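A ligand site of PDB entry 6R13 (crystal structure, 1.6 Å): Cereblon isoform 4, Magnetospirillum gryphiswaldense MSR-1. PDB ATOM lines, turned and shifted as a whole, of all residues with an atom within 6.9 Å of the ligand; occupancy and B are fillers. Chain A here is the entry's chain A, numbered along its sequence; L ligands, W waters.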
ATOM      1  N   VAL A  49      24.068 -31.218 -11.421  1.00  0.00           N
ATOM      2  CA  VAL A  49      24.167 -30.076 -12.307  1.00  0.00           C
ATOM      3  C   VAL A  49      25.606 -29.794 -12.710  1.00  0.00           C
ATOM      4  O   VAL A  49      26.515 -30.224 -12.018  1.00  0.00           O
ATOM      5  CB  VAL A  49      23.548 -28.810 -11.668  1.00  0.00           C
ATOM      6  CG1 VAL A  49      22.032 -29.019 -11.471  1.00  0.00           C
ATOM      7  CG2 VAL A  49      24.241 -28.412 -10.359  1.00  0.00           C
ATOM      8  N   PHE A  50      25.820 -29.053 -13.795  1.00  0.00           N
ATOM      9  CA  PHE A  50      27.175 -28.628 -14.189  1.00  0.00           C
ATOM     10  C   PHE A  50      27.199 -27.132 -14.390  1.00  0.00           C
ATOM     11  O   PHE A  50      26.227 -26.576 -14.926  1.00  0.00           O
ATOM     12  CB  PHE A  50      27.596 -29.226 -15.554  1.00  0.00           C
ATOM     13  CG  PHE A  50      27.669 -30.702 -15.599  1.00  0.00           C
ATOM     14  CD1 PHE A  50      26.529 -31.451 -15.801  1.00  0.00           C
ATOM     15  CD2 PHE A  50      28.878 -31.350 -15.485  1.00  0.00           C
ATOM     16  CE1 PHE A  50      26.600 -32.829 -15.851  1.00  0.00           C
ATOM     17  CE2 PHE A  50      28.974 -32.738 -15.548  1.00  0.00           C
ATOM     18  CZ  PHE A  50      27.819 -33.486 -15.733  1.00  0.00           C
ATOM     19  N   ASN A  51      28.296 -26.500 -13.999  1.00  0.00           N
ATOM     20  CA  ASN A  51      28.498 -25.094 -14.294  1.00  0.00           C
ATOM     21  C   ASN A  51      29.206 -24.887 -15.666  1.00  0.00           C
ATOM     22  O   ASN A  51      29.576 -25.870 -16.331  1.00  0.00           O
ATOM     23  CB  ASN A  51      29.167 -24.396 -13.116  1.00  0.00           C
ATOM     24  CG  ASN A  51      30.640 -24.735 -12.944  1.00  0.00           C
ATOM     25  OD1 ASN A  51      31.276 -25.351 -13.798  1.00  0.00           O
ATOM     26  ND2 ASN A  51      31.191 -24.291 -11.832  1.00  0.00           N
ATOM     27  N   PRO A  52      29.327 -23.624 -16.132  1.00  0.00           N
ATOM     28  CA  PRO A  52      29.963 -23.400 -17.425  1.00  0.00           C
ATOM     29  C   PRO A  52      31.424 -23.844 -17.500  1.00  0.00           C
ATOM     30  O   PRO A  52      31.932 -24.046 -18.591  1.00  0.00           O
ATOM     31  CB  PRO A  52      29.863 -21.890 -17.624  1.00  0.00           C
ATOM     32  CG  PRO A  52      28.707 -21.461 -16.768  1.00  0.00           C
ATOM     33  CD  PRO A  52      28.637 -22.419 -15.633  1.00  0.00           C
ATOM     34  N   ALA A  53      32.079 -23.946 -16.339  1.00  0.00           N
ATOM     35  CA  ALA A  53      33.436 -24.478 -16.253  1.00  0.00           C
ATOM     36  C   ALA A  53      33.509 -25.999 -16.217  1.00  0.00           C
ATOM     37  O   ALA A  53      34.597 -26.549 -16.017  1.00  0.00           O
ATOM     38  CB  ALA A  53      34.133 -23.887 -15.033  1.00  0.00           C
ATOM     39  N   MET A  55      32.321 -28.141 -14.123  1.00  0.00           N
ATOM     40  CA  MET A  55      32.332 -28.774 -12.813  1.00  0.00           C
ATOM     41  C   MET A  55      30.954 -29.335 -12.549  1.00  0.00           C
ATOM     42  O   MET A  55      29.944 -28.614 -12.721  1.00  0.00           O
ATOM     43  CB  MET A  55      32.681 -27.758 -11.732  1.00  0.00           C
ATOM     44  CG  MET A  55      33.998 -27.055 -11.894  1.00  0.00           C
ATOM     45  SD  MET A  55      34.306 -25.977 -10.496  1.00  0.00           S
ATOM     46  CE  MET A  55      33.966 -24.304 -11.035  1.00  0.00           C
ATOM     47  N   PHE A  57      28.189 -30.791  -9.829  1.00  0.00           N
ATOM     48  CA  PHE A  57      27.832 -30.659  -8.436  1.00  0.00           C
ATOM     49  C   PHE A  57      26.615 -31.508  -8.178  1.00  0.00           C
ATOM     50  O   PHE A  57      25.667 -31.483  -8.974  1.00  0.00           O
ATOM     51  CB  PHE A  57      27.514 -29.225  -8.075  1.00  0.00           C
ATOM     52  CG  PHE A  57      28.638 -28.229  -8.344  1.00  0.00           C
ATOM     53  CD1 PHE A  57      29.609 -27.978  -7.406  1.00  0.00           C
ATOM     54  CD2 PHE A  57      28.662 -27.498  -9.517  1.00  0.00           C
ATOM     55  CE1 PHE A  57      30.631 -27.035  -7.651  1.00  0.00           C
ATOM     56  CE2 PHE A  57      29.651 -26.543  -9.745  1.00  0.00           C
ATOM     57  CZ  PHE A  57      30.644 -26.314  -8.817  1.00  0.00           C
ATOM     58  N   SER A  75      22.502 -12.990  -9.484  1.00  0.00           N
ATOM     59  CA  SER A  75      22.564 -13.107 -10.934  1.00  0.00           C
ATOM     60  C   SER A  75      21.630 -14.193 -11.413  1.00  0.00           C
ATOM     61  O   SER A  75      21.556 -15.233 -10.786  1.00  0.00           O
ATOM     62  CB  SER A  75      23.981 -13.463 -11.374  1.00  0.00           C
ATOM     63  OG  SER A  75      23.987 -13.635 -12.800  1.00  0.00           O
ATOM     64  N   GLY A  76      20.963 -13.987 -12.534  1.00  0.00           N
ATOM     65  CA  GLY A  76      20.148 -15.029 -13.160  1.00  0.00           C
ATOM     66  C   GLY A  76      20.920 -15.876 -14.161  1.00  0.00           C
ATOM     67  O   GLY A  76      20.407 -16.886 -14.635  1.00  0.00           O
ATOM     68  N   GLU A  77      22.143 -15.480 -14.468  1.00  0.00           N
ATOM     69  CA  GLU A  77      22.971 -16.137 -15.497  1.00  0.00           C
ATOM     70  C   GLU A  77      23.208 -17.612 -15.193  1.00  0.00           C
ATOM     71  O   GLU A  77      23.674 -17.932 -14.105  1.00  0.00           O
ATOM     72  CB  GLU A  77      24.341 -15.461 -15.603  1.00  0.00           C
ATOM     73  CG  GLU A  77      24.254 -14.017 -16.077  1.00  0.00           C
ATOM     74  CD  GLU A  77      25.488 -13.590 -16.829  1.00  0.00           C
ATOM     75  OE1 GLU A  77      25.358 -13.183 -17.997  1.00  0.00           O
ATOM     76  OE2 GLU A  77      26.599 -13.683 -16.270  1.00  0.00           O
ATOM     77  N   PHE A  78      22.861 -18.474 -16.127  1.00  0.00           N
ATOM     78  CA  PHE A  78      23.084 -19.930 -16.030  1.00  0.00           C
ATOM     79  C   PHE A  78      22.387 -20.583 -14.842  1.00  0.00           C
ATOM     80  O   PHE A  78      22.774 -21.648 -14.430  1.00  0.00           O
ATOM     81  CB  PHE A  78      24.581 -20.275 -15.969  1.00  0.00           C
ATOM     82  CG  PHE A  78      25.420 -19.622 -17.015  1.00  0.00           C
ATOM     83  CD1 PHE A  78      25.333 -20.011 -18.324  1.00  0.00           C
ATOM     84  CD2 PHE A  78      26.339 -18.629 -16.661  1.00  0.00           C
ATOM     85  CE1 PHE A  78      26.154 -19.439 -19.299  1.00  0.00           C
ATOM     86  CE2 PHE A  78      27.158 -18.052 -17.620  1.00  0.00           C
ATOM     87  CZ  PHE A  78      27.070 -18.458 -18.941  1.00  0.00           C
ATOM     88  N   SER A  79      21.311 -19.991 -14.302  1.00  0.00           N
ATOM     89  CA  SER A  79      20.710 -20.552 -13.133  1.00  0.00           C
ATOM     90  C   SER A  79      20.153 -21.922 -13.428  1.00  0.00           C
ATOM     91  O   SER A  79      19.449 -22.127 -14.409  1.00  0.00           O
ATOM     92  CB  SER A  79      19.539 -19.669 -12.624  1.00  0.00           C
ATOM     93  OG  SER A  79      18.994 -20.241 -11.477  1.00  0.00           O
ATOM     94  N   TRP A  80      20.453 -22.854 -12.538  1.00  0.00           N
ATOM     95  CA  TRP A  80      19.932 -24.220 -12.601  1.00  0.00           C
ATOM     96  C   TRP A  80      18.464 -24.346 -12.230  1.00  0.00           C
ATOM     97  O   TRP A  80      17.877 -25.418 -12.431  1.00  0.00           O
ATOM     98  CB  TRP A  80      20.765 -25.118 -11.688  1.00  0.00           C
ATOM     99  CG  TRP A  80      22.185 -25.237 -12.110  1.00  0.00           C
ATOM    100  CD1 TRP A  80      22.670 -25.483 -13.352  1.00  0.00           C
ATOM    101  CD2 TRP A  80      23.312 -25.145 -11.236  1.00  0.00           C
ATOM    102  NE1 TRP A  80      24.055 -25.555 -13.319  1.00  0.00           N
ATOM    103  CE2 TRP A  80      24.470 -25.374 -12.024  1.00  0.00           C
ATOM    104  CE3 TRP A  80      23.468 -24.924  -9.876  1.00  0.00           C
ATOM    105  CZ2 TRP A  80      25.722 -25.353 -11.480  1.00  0.00           C
ATOM    106  CZ3 TRP A  80      24.729 -24.906  -9.336  1.00  0.00           C
ATOM    107  CH2 TRP A  80      25.852 -25.121 -10.157  1.00  0.00           C
ATOM    108  N   PHE A  81      17.868 -23.288 -11.671  1.00  0.00           N
ATOM    109  CA  PHE A  81      16.504 -23.317 -11.193  1.00  0.00           C
ATOM    110  C   PHE A  81      15.769 -22.146 -11.810  1.00  0.00           C
ATOM    111  O   PHE A  81      16.105 -20.987 -11.562  1.00  0.00           O
ATOM    112  CB  PHE A  81      16.487 -23.248  -9.663  1.00  0.00           C
ATOM    113  CG  PHE A  81      17.230 -24.375  -9.017  1.00  0.00           C
ATOM    114  CD1 PHE A  81      16.601 -25.589  -8.821  1.00  0.00           C
ATOM    115  CD2 PHE A  81      18.529 -24.225  -8.617  1.00  0.00           C
ATOM    116  CE1 PHE A  81      17.250 -26.636  -8.208  1.00  0.00           C
ATOM    117  CE2 PHE A  81      19.203 -25.281  -8.017  1.00  0.00           C
ATOM    118  CZ  PHE A  81      18.557 -26.489  -7.813  1.00  0.00           C
ATOM    119  N   TYR A  84      14.880 -18.226 -10.639  1.00  0.00           N
ATOM    120  CA  TYR A  84      15.706 -17.828  -9.487  1.00  0.00           C
ATOM    121  C   TYR A  84      17.023 -17.239  -9.892  1.00  0.00           C
ATOM    122  O   TYR A  84      17.608 -17.655 -10.903  1.00  0.00           O
ATOM    123  CB  TYR A  84      15.971 -19.015  -8.595  1.00  0.00           C
ATOM    124  CG  TYR A  84      14.761 -19.605  -7.979  1.00  0.00           C
ATOM    125  CD1 TYR A  84      14.280 -19.144  -6.772  1.00  0.00           C
ATOM    126  CD2 TYR A  84      14.089 -20.632  -8.590  1.00  0.00           C
ATOM    127  CE1 TYR A  84      13.162 -19.722  -6.168  1.00  0.00           C
ATOM    128  CE2 TYR A  84      12.975 -21.220  -8.020  1.00  0.00           C
ATOM    129  CZ  TYR A  84      12.497 -20.721  -6.812  1.00  0.00           C
ATOM    130  OH  TYR A  84      11.388 -21.283  -6.249  1.00  0.00           O
ATOM    131  N   TRP A  86      20.884 -16.264  -8.335  1.00  0.00           N
ATOM    132  CA  TRP A  86      21.767 -16.882  -7.321  1.00  0.00           C
ATOM    133  C   TRP A  86      22.853 -15.923  -6.844  1.00  0.00           C
ATOM    134  O   TRP A  86      23.259 -15.008  -7.563  1.00  0.00           O
ATOM    135  CB  TRP A  86      22.425 -18.152  -7.858  1.00  0.00           C
ATOM    136  CG  TRP A  86      23.131 -17.984  -9.157  1.00  0.00           C
ATOM    137  CD1 TRP A  86      22.608 -18.219 -10.390  1.00  0.00           C
ATOM    138  CD2 TRP A  86      24.482 -17.524  -9.375  1.00  0.00           C
ATOM    139  NE1 TRP A  86      23.528 -17.907 -11.349  1.00  0.00           N
ATOM    140  CE2 TRP A  86      24.679 -17.459 -10.764  1.00  0.00           C
ATOM    141  CE3 TRP A  86      25.542 -17.113  -8.519  1.00  0.00           C
ATOM    142  CZ2 TRP A  86      25.869 -17.034 -11.319  1.00  0.00           C
ATOM    143  CZ3 TRP A  86      26.722 -16.680  -9.078  1.00  0.00           C
ATOM    144  CH2 TRP A  86      26.886 -16.674 -10.465  1.00  0.00           C
ATOM    145  N   THR A  87      23.308 -16.183  -5.611  1.00  0.00           N
ATOM    146  CA  THR A  87      24.494 -15.547  -5.025  1.00  0.00           C
ATOM    147  C   THR A  87      25.327 -16.678  -4.453  1.00  0.00           C
ATOM    148  O   THR A  87      24.800 -17.656  -3.926  1.00  0.00           O
ATOM    149  CB  THR A  87      24.198 -14.561  -3.887  1.00  0.00           C
ATOM    150  OG1 THR A  87      23.355 -15.177  -2.901  1.00  0.00           O
ATOM    151  CG2 THR A  87      23.559 -13.270  -4.428  1.00  0.00           C
ATOM    152  N   ILE A  88      26.643 -16.542  -4.569  1.00  0.00           N
ATOM    153  CA  ILE A  88      27.556 -17.532  -3.990  1.00  0.00           C
ATOM    154  C   ILE A  88      27.409 -17.518  -2.469  1.00  0.00           C
ATOM    155  O   ILE A  88      27.376 -16.430  -1.847  1.00  0.00           O
ATOM    156  CB  ILE A  88      29.004 -17.187  -4.375  1.00  0.00           C
ATOM    157  CG1 ILE A  88      29.170 -17.439  -5.871  1.00  0.00           C
ATOM    158  CG2 ILE A  88      30.013 -17.989  -3.560  1.00  0.00           C
ATOM    159  CD1 ILE A  88      30.371 -16.706  -6.446  1.00  0.00           C
ATOM    160  N   HIS A  97      33.579 -22.645  -0.248  1.00  0.00           N
ATOM    161  CA  HIS A  97      32.373 -22.448  -1.097  1.00  0.00           C
ATOM    162  C   HIS A  97      31.409 -23.595  -0.911  1.00  0.00           C
ATOM    163  O   HIS A  97      31.668 -24.712  -1.345  1.00  0.00           O
ATOM    164  CB  HIS A  97      32.775 -22.307  -2.556  1.00  0.00           C
ATOM    165  CG  HIS A  97      31.600 -22.183  -3.453  1.00  0.00           C
ATOM    166  ND1 HIS A  97      31.619 -22.647  -4.752  1.00  0.00           N
ATOM    167  CD2 HIS A  97      30.368 -21.668  -3.256  1.00  0.00           C
ATOM    168  CE1 HIS A  97      30.459 -22.382  -5.326  1.00  0.00           C
ATOM    169  NE2 HIS A  97      29.665 -21.830  -4.431  1.00  0.00           N
ATOM    170  N   TRP A 100      25.030 -22.038  -3.066  1.00  0.00           N
ATOM    171  CA  TRP A 100      24.410 -20.808  -3.593  1.00  0.00           C
ATOM    172  C   TRP A 100      23.109 -20.551  -2.851  1.00  0.00           C
ATOM    173  O   TRP A 100      22.452 -21.472  -2.414  1.00  0.00           O
ATOM    174  CB  TRP A 100      24.092 -20.944  -5.079  1.00  0.00           C
ATOM    175  CG  TRP A 100      25.324 -21.264  -5.912  1.00  0.00           C
ATOM    176  CD1 TRP A 100      26.145 -20.370  -6.495  1.00  0.00           C
ATOM    177  CD2 TRP A 100      25.915 -22.553  -6.122  1.00  0.00           C
ATOM    178  NE1 TRP A 100      27.205 -21.026  -7.090  1.00  0.00           N
ATOM    179  CE2 TRP A 100      27.057 -22.368  -6.900  1.00  0.00           C
ATOM    180  CE3 TRP A 100      25.551 -23.849  -5.760  1.00  0.00           C
ATOM    181  CZ2 TRP A 100      27.871 -23.432  -7.327  1.00  0.00           C
ATOM    182  CZ3 TRP A 100      26.359 -24.915  -6.175  1.00  0.00           C
ATOM    183  CH2 TRP A 100      27.516 -24.684  -6.935  1.00  0.00           C
ATOM    184  N   TYR A 102      19.422 -18.859  -3.570  1.00  0.00           N
ATOM    185  CA  TYR A 102      18.535 -18.548  -4.690  1.00  0.00           C
ATOM    186  C   TYR A 102      17.413 -17.660  -4.203  1.00  0.00           C
ATOM    187  O   TYR A 102      16.920 -17.843  -3.103  1.00  0.00           O
ATOM    188  CB  TYR A 102      17.972 -19.838  -5.290  1.00  0.00           C
ATOM    189  CG  TYR A 102      19.034 -20.616  -6.023  1.00  0.00           C
ATOM    190  CD1 TYR A 102      19.314 -20.350  -7.351  1.00  0.00           C
ATOM    191  CD2 TYR A 102      19.780 -21.548  -5.351  1.00  0.00           C
ATOM    192  CE1 TYR A 102      20.317 -21.083  -8.024  1.00  0.00           C
ATOM    193  CE2 TYR A 102      20.773 -22.297  -6.009  1.00  0.00           C
ATOM    194  CZ  TYR A 102      21.041 -22.017  -7.324  1.00  0.00           C
ATOM    195  OH  TYR A 102      22.020 -22.721  -7.996  1.00  0.00           O
HETATM  196  O1  LIG L   1      26.200 -22.488 -13.202  1.00  0.00           O
HETATM  197  C1  LIG L   1      25.760 -22.039 -12.139  1.00  0.00           C
HETATM  198  N1  LIG L   1      24.424 -22.048 -12.016  1.00  0.00           N
HETATM  199  C2  LIG L   1      23.811 -21.750 -10.832  1.00  0.00           C
HETATM  200  O2  LIG L   1      22.626 -21.876 -10.628  1.00  0.00           O
HETATM  201  C3  LIG L   1      24.688 -21.299  -9.691  1.00  0.00           C
HETATM  202  C4  LIG L   1      25.914 -20.574 -10.165  1.00  0.00           C
HETATM  203  C5  LIG L   1      26.564 -21.367 -11.237  1.00  0.00           C
HETATM  204  N2  LIG L   1      27.846 -21.040 -11.608  1.00  0.00           N
HETATM  205  C6  LIG L   1      32.218 -20.047 -12.887  1.00  0.00           C
HETATM  206  C7  LIG L   1      31.496 -20.946 -12.081  1.00  0.00           C
HETATM  207  C8  LIG L   1      30.091 -20.835 -12.019  1.00  0.00           C
HETATM  208  C9  LIG L   1      29.406 -19.864 -12.740  1.00  0.00           C
HETATM  209  O3  LIG L   1      29.179 -22.534 -10.526  1.00  0.00           O
HETATM  210  O4  LIG L   1      26.896 -19.517 -13.311  1.00  0.00           O
HETATM  211  C10 LIG L   1      30.122 -18.944 -13.504  1.00  0.00           C
HETATM  212  C11 LIG L   1      31.523 -19.043 -13.582  1.00  0.00           C
HETATM  213  C12 LIG L   1      27.969 -19.832 -12.426  1.00  0.00           C
HETATM  214  C13 LIG L   1      29.018 -21.573 -11.278  1.00  0.00           C
HETATM  215  O   HOH W   1      27.819 -16.384 -13.908  1.00  0.00           O
HETATM  216  O   HOH W   2      29.208 -19.596  -8.772  1.00  0.00           O
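N1 of the ligand is in hydrogen-bond range of O of Phe 78 (3.0 Å). An oxygen (O2) of the ligand sits at hydrogen-bond distance from the side-chain hydroxyl (OH) of Tyr 102. An oxygen (O3) of the ligand lies within hydrogen-bond range of the side-chain amide nitrogen (ND2) of Asn 51. The backbone NH (N) of Trp 80 lies within hydrogen-bond range of an oxygen (O2) of the ligand.
The indole nitrogen (NE1) of Trp 80 is in hydrogen-bond range of the backbone carbonyl oxygen (O) of Phe 50 (2.9 Å). N of Glu 77 sits at hydrogen-bond distance from OG of Ser 75 (3.1 Å). The side-chain hydroxyl (OG) of Ser 79 lies within hydrogen-bond range of the backbone carbonyl oxygen (O) of Tyr 84 (3.0 Å). The backbone carbonyl oxygen (O) of Glu 77 sits at hydrogen-bond distance from the indole nitrogen (NE1) of Trp 86, at 2.8 Å. The backbone NH (N) of Met 55 sits at hydrogen-bond distance from the side-chain amide oxygen (OD1) of Asn 51 (3.0 Å). The backbone carbonyl oxygen (O) of Phe 81 lies within hydrogen-bond range of the side-chain hydroxyl (OG) of Ser 79, 3.0 Å away. The backbone NH (N) of Trp 86 sits at hydrogen-bond distance from the backbone carbonyl oxygen (O) of Ser 75 (2.7 Å). The side-chain amide oxygen of Asn 51 lies within hydrogen-bond range of the backbone NH of Ala 53, at 3.0 Å.
CD of Pro 52 touches O1 of the ligand (3.4 Å). Glu 77 touches the ligand (O to O4, 3.7 Å). Ser 79 touches the ligand. Trp 86 touches the ligand. Trp 100 touches the ligand (NE1 to C4, 3.4 Å). Hydrophobic or aromatic side chains that line the ligand: Pro 52, Phe 78, Trp 80, Trp 86, Trp 100 and Tyr 102. Nine residues have an atom within 4 Å of the ligand: Asn 51, Pro 52, Glu 77, Phe 78, Ser 79, Trp 80, Trp 86, Trp 100 and Tyr 102.
Water W2 lies within hydrogen-bond range of the indole nitrogen of Trp 100 (3.0 Å) and an oxygen (O3) of the ligand (3.4 Å).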
